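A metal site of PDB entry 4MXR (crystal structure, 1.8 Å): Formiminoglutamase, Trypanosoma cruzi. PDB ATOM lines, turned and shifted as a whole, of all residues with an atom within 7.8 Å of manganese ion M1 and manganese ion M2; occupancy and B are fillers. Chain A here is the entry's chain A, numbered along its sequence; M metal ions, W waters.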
ATOM      1  N   ASN A  46      37.434  25.862 -19.945  1.00  0.00           N
ATOM      2  CA  ASN A  46      36.731  25.007 -20.903  1.00  0.00           C
ATOM      3  C   ASN A  46      35.898  25.855 -21.860  1.00  0.00           C
ATOM      4  O   ASN A  46      35.107  25.330 -22.642  1.00  0.00           O
ATOM      5  CB  ASN A  46      35.843  24.007 -20.156  1.00  0.00           C
ATOM      6  CG  ASN A  46      35.401  22.840 -21.027  1.00  0.00           C
ATOM      7  OD1 ASN A  46      36.025  22.534 -22.049  1.00  0.00           O
ATOM      8  ND2 ASN A  46      34.335  22.173 -20.614  1.00  0.00           N
ATOM      9  N   GLY A 121      32.438  24.241 -10.859  1.00  0.00           N
ATOM     10  CA  GLY A 121      32.649  23.576 -12.144  1.00  0.00           C
ATOM     11  C   GLY A 121      32.875  22.078 -12.037  1.00  0.00           C
ATOM     12  O   GLY A 121      33.283  21.577 -10.992  1.00  0.00           O
ATOM     13  N   ASN A 122      32.634  21.373 -13.136  1.00  0.00           N
ATOM     14  CA  ASN A 122      32.717  19.922 -13.168  1.00  0.00           C
ATOM     15  C   ASN A 122      34.124  19.364 -12.915  1.00  0.00           C
ATOM     16  O   ASN A 122      34.291  18.163 -12.691  1.00  0.00           O
ATOM     17  CB  ASN A 122      32.176  19.384 -14.500  1.00  0.00           C
ATOM     18  CG  ASN A 122      31.371  18.104 -14.333  1.00  0.00           C
ATOM     19  OD1 ASN A 122      30.438  17.859 -15.094  1.00  0.00           O
ATOM     20  ND2 ASN A 122      31.718  17.298 -13.343  1.00  0.00           N
ATOM     21  N   ASP A 123      35.136  20.226 -12.951  1.00  0.00           N
ATOM     22  CA  ASP A 123      36.497  19.794 -12.634  1.00  0.00           C
ATOM     23  C   ASP A 123      36.586  19.212 -11.224  1.00  0.00           C
ATOM     24  O   ASP A 123      37.520  18.470 -10.917  1.00  0.00           O
ATOM     25  CB  ASP A 123      37.510  20.931 -12.816  1.00  0.00           C
ATOM     26  CG  ASP A 123      37.032  22.243 -12.223  1.00  0.00           C
ATOM     27  OD1 ASP A 123      36.107  22.864 -12.793  1.00  0.00           O
ATOM     28  OD2 ASP A 123      37.601  22.670 -11.193  1.00  0.00           O
ATOM     29  N   SER A 125      35.008  16.873 -10.106  1.00  0.00           N
ATOM     30  CA  SER A 125      34.782  15.429 -10.170  1.00  0.00           C
ATOM     31  C   SER A 125      36.068  14.615 -10.239  1.00  0.00           C
ATOM     32  O   SER A 125      36.081  13.454  -9.842  1.00  0.00           O
ATOM     33  CB  SER A 125      33.851  15.089 -11.331  1.00  0.00           C
ATOM     34  OG  SER A 125      32.637  15.801 -11.204  1.00  0.00           O
ATOM     35  N   ASN A 144      28.764   9.369 -14.835  1.00  0.00           N
ATOM     36  CA  ASN A 144      28.683  10.796 -15.111  1.00  0.00           C
ATOM     37  C   ASN A 144      27.370  11.153 -15.795  1.00  0.00           C
ATOM     38  O   ASN A 144      27.189  10.895 -16.984  1.00  0.00           O
ATOM     39  CB  ASN A 144      29.865  11.257 -15.978  1.00  0.00           C
ATOM     40  CG  ASN A 144      29.784  12.736 -16.305  1.00  0.00           C
ATOM     41  OD1 ASN A 144      29.278  13.526 -15.523  1.00  0.00           O
ATOM     42  ND2 ASN A 144      30.275  13.118 -17.490  1.00  0.00           N
ATOM     43  N   VAL A 145      26.447  11.705 -15.025  1.00  0.00           N
ATOM     44  CA  VAL A 145      25.197  12.181 -15.593  1.00  0.00           C
ATOM     45  C   VAL A 145      25.468  13.558 -16.190  1.00  0.00           C
ATOM     46  O   VAL A 145      25.721  14.528 -15.452  1.00  0.00           O
ATOM     47  CB  VAL A 145      24.079  12.272 -14.541  1.00  0.00           C
ATOM     48  CG1 VAL A 145      22.752  12.664 -15.207  1.00  0.00           C
ATOM     49  CG2 VAL A 145      23.947  10.946 -13.804  1.00  0.00           C
ATOM     50  N   ASP A 146      25.424  13.639 -17.507  1.00  0.00           N
ATOM     51  CA  ASP A 146      25.921  14.816 -18.204  1.00  0.00           C
ATOM     52  C   ASP A 146      25.511  14.740 -19.676  1.00  0.00           C
ATOM     53  O   ASP A 146      25.548  13.667 -20.280  1.00  0.00           O
ATOM     54  CB  ASP A 146      27.447  14.813 -18.099  1.00  0.00           C
ATOM     55  CG  ASP A 146      28.053  16.167 -18.371  1.00  0.00           C
ATOM     56  OD1 ASP A 146      27.440  16.976 -19.094  1.00  0.00           O
ATOM     57  OD2 ASP A 146      29.156  16.410 -17.857  1.00  0.00           O
ATOM     58  N   SER A 147      25.122  15.870 -20.250  1.00  0.00           N
ATOM     59  CA  SER A 147      24.875  15.920 -21.683  1.00  0.00           C
ATOM     60  C   SER A 147      26.191  15.812 -22.450  1.00  0.00           C
ATOM     61  O   SER A 147      26.198  15.470 -23.636  1.00  0.00           O
ATOM     62  CB  SER A 147      24.131  17.210 -22.067  1.00  0.00           C
ATOM     63  OG  SER A 147      24.838  18.347 -21.622  1.00  0.00           O
ATOM     64  N   HIS A 148      27.304  16.110 -21.773  1.00  0.00           N
ATOM     65  CA  HIS A 148      28.635  16.045 -22.383  1.00  0.00           C
ATOM     66  C   HIS A 148      29.476  14.926 -21.764  1.00  0.00           C
ATOM     67  O   HIS A 148      29.238  14.509 -20.633  1.00  0.00           O
ATOM     68  CB  HIS A 148      29.361  17.384 -22.208  1.00  0.00           C
ATOM     69  CG  HIS A 148      28.480  18.571 -22.442  1.00  0.00           C
ATOM     70  ND1 HIS A 148      27.850  19.248 -21.416  1.00  0.00           N
ATOM     71  CD2 HIS A 148      28.103  19.197 -23.585  1.00  0.00           C
ATOM     72  CE1 HIS A 148      27.133  20.243 -21.914  1.00  0.00           C
ATOM     73  NE2 HIS A 148      27.273  20.231 -23.229  1.00  0.00           N
ATOM     74  N   LEU A 149      30.465  14.443 -22.516  1.00  0.00           N
ATOM     75  CA  LEU A 149      31.299  13.330 -22.041  1.00  0.00           C
ATOM     76  C   LEU A 149      32.363  13.776 -21.039  1.00  0.00           C
ATOM     77  O   LEU A 149      32.736  13.019 -20.135  1.00  0.00           O
ATOM     78  CB  LEU A 149      31.946  12.609 -23.228  1.00  0.00           C
ATOM     79  CG  LEU A 149      31.014  11.879 -24.202  1.00  0.00           C
ATOM     80  CD1 LEU A 149      31.812  11.040 -25.175  1.00  0.00           C
ATOM     81  CD2 LEU A 149      30.027  11.022 -23.431  1.00  0.00           C
ATOM     82  N   ASP A 150      32.865  14.990 -21.210  1.00  0.00           N
ATOM     83  CA  ASP A 150      33.879  15.551 -20.319  1.00  0.00           C
ATOM     84  C   ASP A 150      35.146  14.694 -20.290  1.00  0.00           C
ATOM     85  O   ASP A 150      35.702  14.414 -19.223  1.00  0.00           O
ATOM     86  CB  ASP A 150      33.330  15.717 -18.908  1.00  0.00           C
ATOM     87  CG  ASP A 150      32.428  16.926 -18.781  1.00  0.00           C
ATOM     88  OD1 ASP A 150      32.073  17.527 -19.827  1.00  0.00           O
ATOM     89  OD2 ASP A 150      32.074  17.279 -17.632  1.00  0.00           O
ATOM     90  N   SER A 162      36.844  22.060 -16.604  1.00  0.00           N
ATOM     91  CA  SER A 162      35.559  21.422 -16.371  1.00  0.00           C
ATOM     92  C   SER A 162      35.247  20.328 -17.389  1.00  0.00           C
ATOM     93  O   SER A 162      34.307  19.554 -17.205  1.00  0.00           O
ATOM     94  CB  SER A 162      34.425  22.459 -16.361  1.00  0.00           C
ATOM     95  OG  SER A 162      34.306  23.103 -17.622  1.00  0.00           O
ATOM     96  N   GLY A 163      36.034  20.260 -18.458  1.00  0.00           N
ATOM     97  CA  GLY A 163      35.799  19.294 -19.512  1.00  0.00           C
ATOM     98  C   GLY A 163      36.705  18.074 -19.518  1.00  0.00           C
ATOM     99  O   GLY A 163      36.592  17.212 -20.383  1.00  0.00           O
ATOM    100  N   THR A 164      37.607  17.990 -18.547  1.00  0.00           N
ATOM    101  CA  THR A 164      38.583  16.899 -18.517  1.00  0.00           C
ATOM    102  C   THR A 164      38.427  15.885 -17.387  1.00  0.00           C
ATOM    103  O   THR A 164      39.184  14.909 -17.347  1.00  0.00           O
ATOM    104  CB  THR A 164      40.022  17.445 -18.437  1.00  0.00           C
ATOM    105  OG1 THR A 164      40.258  17.998 -17.136  1.00  0.00           O
ATOM    106  CG2 THR A 164      40.263  18.501 -19.498  1.00  0.00           C
ATOM    107  N   PRO A 165      37.469  16.089 -16.470  1.00  0.00           N
ATOM    108  CA  PRO A 165      37.553  15.260 -15.257  1.00  0.00           C
ATOM    109  C   PRO A 165      37.497  13.758 -15.497  1.00  0.00           C
ATOM    110  O   PRO A 165      38.156  13.009 -14.785  1.00  0.00           O
ATOM    111  CB  PRO A 165      36.334  15.712 -14.437  1.00  0.00           C
ATOM    112  CG  PRO A 165      35.380  16.226 -15.455  1.00  0.00           C
ATOM    113  CD  PRO A 165      36.251  16.911 -16.475  1.00  0.00           C
ATOM    114  N   PHE A 166      36.740  13.312 -16.496  1.00  0.00           N
ATOM    115  CA  PHE A 166      36.576  11.877 -16.688  1.00  0.00           C
ATOM    116  C   PHE A 166      37.632  11.255 -17.609  1.00  0.00           C
ATOM    117  O   PHE A 166      37.798  10.032 -17.634  1.00  0.00           O
ATOM    118  CB  PHE A 166      35.140  11.521 -17.059  1.00  0.00           C
ATOM    119  CG  PHE A 166      34.157  11.963 -16.015  1.00  0.00           C
ATOM    120  CD1 PHE A 166      33.964  11.200 -14.874  1.00  0.00           C
ATOM    121  CD2 PHE A 166      33.486  13.167 -16.129  1.00  0.00           C
ATOM    122  CE1 PHE A 166      33.091  11.609 -13.889  1.00  0.00           C
ATOM    123  CE2 PHE A 166      32.613  13.588 -15.152  1.00  0.00           C
ATOM    124  CZ  PHE A 166      32.405  12.801 -14.025  1.00  0.00           C
ATOM    125  N   GLU A 182      28.643   6.978 -18.974  1.00  0.00           N
ATOM    126  CA  GLU A 182      28.232   8.315 -19.375  1.00  0.00           C
ATOM    127  C   GLU A 182      26.721   8.260 -19.552  1.00  0.00           C
ATOM    128  O   GLU A 182      26.224   7.589 -20.469  1.00  0.00           O
ATOM    129  CB  GLU A 182      28.901   8.706 -20.694  1.00  0.00           C
ATOM    130  CG  GLU A 182      30.425   8.800 -20.646  1.00  0.00           C
ATOM    131  CD  GLU A 182      30.939  10.129 -20.118  1.00  0.00           C
ATOM    132  OE1 GLU A 182      30.171  10.854 -19.438  1.00  0.00           O
ATOM    133  OE2 GLU A 182      32.121  10.463 -20.376  1.00  0.00           O
ATOM    134  N   GLN A 189      26.191  16.943 -29.017  1.00  0.00           N
ATOM    135  CA  GLN A 189      27.185  17.683 -28.239  1.00  0.00           C
ATOM    136  C   GLN A 189      28.435  16.854 -27.953  1.00  0.00           C
ATOM    137  O   GLN A 189      29.379  17.350 -27.351  1.00  0.00           O
ATOM    138  CB  GLN A 189      26.585  18.132 -26.903  1.00  0.00           C
ATOM    139  CG  GLN A 189      25.192  18.750 -26.968  1.00  0.00           C
ATOM    140  CD  GLN A 189      24.885  19.581 -25.734  1.00  0.00           C
ATOM    141  OE1 GLN A 189      25.549  20.592 -25.473  1.00  0.00           O
ATOM    142  NE2 GLN A 189      23.873  19.181 -24.977  1.00  0.00           N
ATOM    143  N   SER A 234      27.868  11.131 -10.040  1.00  0.00           N
ATOM    144  CA  SER A 234      28.360  12.457 -10.397  1.00  0.00           C
ATOM    145  C   SER A 234      27.387  13.153 -11.355  1.00  0.00           C
ATOM    146  O   SER A 234      27.232  12.724 -12.489  1.00  0.00           O
ATOM    147  CB  SER A 234      29.745  12.335 -11.050  1.00  0.00           C
ATOM    148  OG  SER A 234      30.337  13.604 -11.299  1.00  0.00           O
ATOM    149  N   PHE A 235      26.747  14.211 -10.880  1.00  0.00           N
ATOM    150  CA  PHE A 235      25.620  14.804 -11.589  1.00  0.00           C
ATOM    151  C   PHE A 235      25.901  16.225 -12.083  1.00  0.00           C
ATOM    152  O   PHE A 235      25.883  17.176 -11.313  1.00  0.00           O
ATOM    153  CB  PHE A 235      24.389  14.811 -10.676  1.00  0.00           C
ATOM    154  CG  PHE A 235      23.083  14.652 -11.414  1.00  0.00           C
ATOM    155  CD1 PHE A 235      22.806  15.401 -12.547  1.00  0.00           C
ATOM    156  CD2 PHE A 235      22.129  13.740 -10.964  1.00  0.00           C
ATOM    157  CE1 PHE A 235      21.594  15.258 -13.207  1.00  0.00           C
ATOM    158  CE2 PHE A 235      20.926  13.594 -11.628  1.00  0.00           C
ATOM    159  CZ  PHE A 235      20.665  14.346 -12.756  1.00  0.00           C
ATOM    160  N   ASP A 236      26.164  16.357 -13.380  1.00  0.00           N
ATOM    161  CA  ASP A 236      26.292  17.665 -14.007  1.00  0.00           C
ATOM    162  C   ASP A 236      24.893  18.150 -14.357  1.00  0.00           C
ATOM    163  O   ASP A 236      24.260  17.581 -15.235  1.00  0.00           O
ATOM    164  CB  ASP A 236      27.147  17.550 -15.272  1.00  0.00           C
ATOM    165  CG  ASP A 236      27.291  18.870 -16.004  1.00  0.00           C
ATOM    166  OD1 ASP A 236      26.455  19.774 -15.828  1.00  0.00           O
ATOM    167  OD2 ASP A 236      28.259  19.017 -16.771  1.00  0.00           O
ATOM    168  N   VAL A 237      24.421  19.182 -13.667  1.00  0.00           N
ATOM    169  CA  VAL A 237      23.029  19.613 -13.844  1.00  0.00           C
ATOM    170  C   VAL A 237      22.710  20.192 -15.223  1.00  0.00           C
ATOM    171  O   VAL A 237      21.553  20.515 -15.494  1.00  0.00           O
ATOM    172  CB  VAL A 237      22.541  20.579 -12.735  1.00  0.00           C
ATOM    173  CG1 VAL A 237      22.504  19.871 -11.380  1.00  0.00           C
ATOM    174  CG2 VAL A 237      23.420  21.825 -12.682  1.00  0.00           C
ATOM    175  N   ASP A 238      23.700  20.306 -16.102  1.00  0.00           N
ATOM    176  CA  ASP A 238      23.387  20.749 -17.462  1.00  0.00           C
ATOM    177  C   ASP A 238      22.891  19.579 -18.321  1.00  0.00           C
ATOM    178  O   ASP A 238      22.692  19.723 -19.525  1.00  0.00           O
ATOM    179  CB  ASP A 238      24.535  21.533 -18.111  1.00  0.00           C
ATOM    180  CG  ASP A 238      25.712  20.657 -18.520  1.00  0.00           C
ATOM    181  OD1 ASP A 238      25.524  19.448 -18.772  1.00  0.00           O
ATOM    182  OD2 ASP A 238      26.823  21.208 -18.615  1.00  0.00           O
ATOM    183  N   SER A 239      22.714  18.429 -17.676  1.00  0.00           N
ATOM    184  CA  SER A 239      22.065  17.280 -18.312  1.00  0.00           C
ATOM    185  C   SER A 239      20.554  17.466 -18.314  1.00  0.00           C
ATOM    186  O   SER A 239      19.838  16.760 -19.032  1.00  0.00           O
ATOM    187  CB  SER A 239      22.430  15.979 -17.580  1.00  0.00           C
ATOM    188  OG  SER A 239      22.045  16.037 -16.221  1.00  0.00           O
ATOM    189  N   VAL A 248      22.817  27.251 -15.878  1.00  0.00           N
ATOM    190  CA  VAL A 248      24.091  26.550 -16.074  1.00  0.00           C
ATOM    191  C   VAL A 248      24.867  27.244 -17.187  1.00  0.00           C
ATOM    192  O   VAL A 248      24.283  27.959 -18.001  1.00  0.00           O
ATOM    193  CB  VAL A 248      23.868  25.077 -16.483  1.00  0.00           C
ATOM    194  CG1 VAL A 248      23.235  24.293 -15.361  1.00  0.00           C
ATOM    195  CG2 VAL A 248      23.019  25.006 -17.748  1.00  0.00           C
ATOM    196  N   CYS A 250      26.303  25.886 -19.801  1.00  0.00           N
ATOM    197  CA  CYS A 250      25.920  25.334 -21.094  1.00  0.00           C
ATOM    198  C   CYS A 250      24.500  24.781 -21.047  1.00  0.00           C
ATOM    199  O   CYS A 250      24.290  23.586 -20.827  1.00  0.00           O
ATOM    200  CB  CYS A 250      26.914  24.246 -21.506  1.00  0.00           C
ATOM    201  SG  CYS A 250      26.793  23.767 -23.244  1.00  0.00           S
ATOM    202  N   SER A 280      27.591  19.419 -10.275  1.00  0.00           N
ATOM    203  CA  SER A 280      28.390  20.463 -10.888  1.00  0.00           C
ATOM    204  C   SER A 280      27.605  21.385 -11.817  1.00  0.00           C
ATOM    205  O   SER A 280      26.540  21.017 -12.321  1.00  0.00           O
ATOM    206  CB  SER A 280      29.540  19.841 -11.701  1.00  0.00           C
ATOM    207  OG  SER A 280      30.271  18.913 -10.933  1.00  0.00           O
ATOM    208  N   GLU A 281      28.146  22.581 -12.034  1.00  0.00           N
ATOM    209  CA  GLU A 281      27.727  23.502 -13.090  1.00  0.00           C
ATOM    210  C   GLU A 281      26.541  24.410 -12.781  1.00  0.00           C
ATOM    211  O   GLU A 281      26.096  25.166 -13.643  1.00  0.00           O
ATOM    212  CB  GLU A 281      27.490  22.747 -14.415  1.00  0.00           C
ATOM    213  CG  GLU A 281      28.731  22.021 -14.960  1.00  0.00           C
ATOM    214  CD  GLU A 281      29.832  22.980 -15.380  1.00  0.00           C
ATOM    215  OE1 GLU A 281      29.518  23.998 -16.037  1.00  0.00           O
ATOM    216  OE2 GLU A 281      31.014  22.705 -15.068  1.00  0.00           O
HETATM  217 MN    MN M   1      30.212  18.191 -17.207  1.00  0.00          MN
HETATM  218 MN    MN M   2      27.768  19.124 -19.119  1.00  0.00          MN
HETATM  219  O   HOH W   1      31.455  20.306 -17.280  1.00  0.00           O
HETATM  220  O   HOH W   2      30.124  19.191 -19.276  1.00  0.00           O
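The backbone carbonyl oxygen of Asp 150 lies within hydrogen-bond range of the backbone NH of Phe 166 (3.1 Å).
ND2 of Asn 122 sits at hydrogen-bond distance from OG of Ser 280 (3.2 Å).
OG of Ser 125 is in hydrogen-bond range of ND2 of Asn 122 (2.8 Å).
O of Asp 236 lies within hydrogen-bond range of OG of Ser 239 (2.9 Å).
The backbone carbonyl oxygen of Val 145 sits at hydrogen-bond distance from the backbone NH of Asp 236, at 2.8 Å.
ND2 of Asn 144 sits close to OD2 of Asp 146, 3.5 Å away.
A ring nitrogen (NE2) of His 148 lies close to the side-chain hydroxyl (OG) of Ser 147 (3.5 Å).
SG of Cys 250 sits at hydrogen-bond distance from NE2 of His 148, at 3.6 Å.
Four residues have an atom within 4 Å of manganese ion M1: Asn 122, Asp 146, Asp 150 and Asp 236.
The nearest printed residue that does not touch manganese ion M1 is Ser 162 (4.3 Å).
Residues that only touch manganese ion M2: Ser 147.
Along chain A the residues within 4 Å of manganese ion M2 span positions 146 to 238.
The nearest printed residue that does not touch manganese ion M2 is Asp 150 (4.6 Å).
The side-chain carboxylate (OD2) of Asp 150 binds manganese ion M1 (2.1 Å).
The side-chain amide oxygen (OD1) of Asn 122 binds manganese ion M1 (2.2 Å).
OD2 of Asp 236 binds manganese ion M1, at 2.2 Å.
Manganese ion M1 is bound by OD2 of Asp 146 (2.2 Å).
Water W2 is bound to manganese ion M1 (2.3 Å).
Water W1 binds manganese ion M1, 2.5 Å away.
Manganese ion M2 is bound by OD1 of Asp 146, OD1 of Asp 238, ND1 of His 148, OD2 of Asp 238, water W2 and OD2 of Asp 236.
Water W1 bridges O of Ser 162 (3.0 Å) and OE2 of Glu 281 (3.3 Å).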
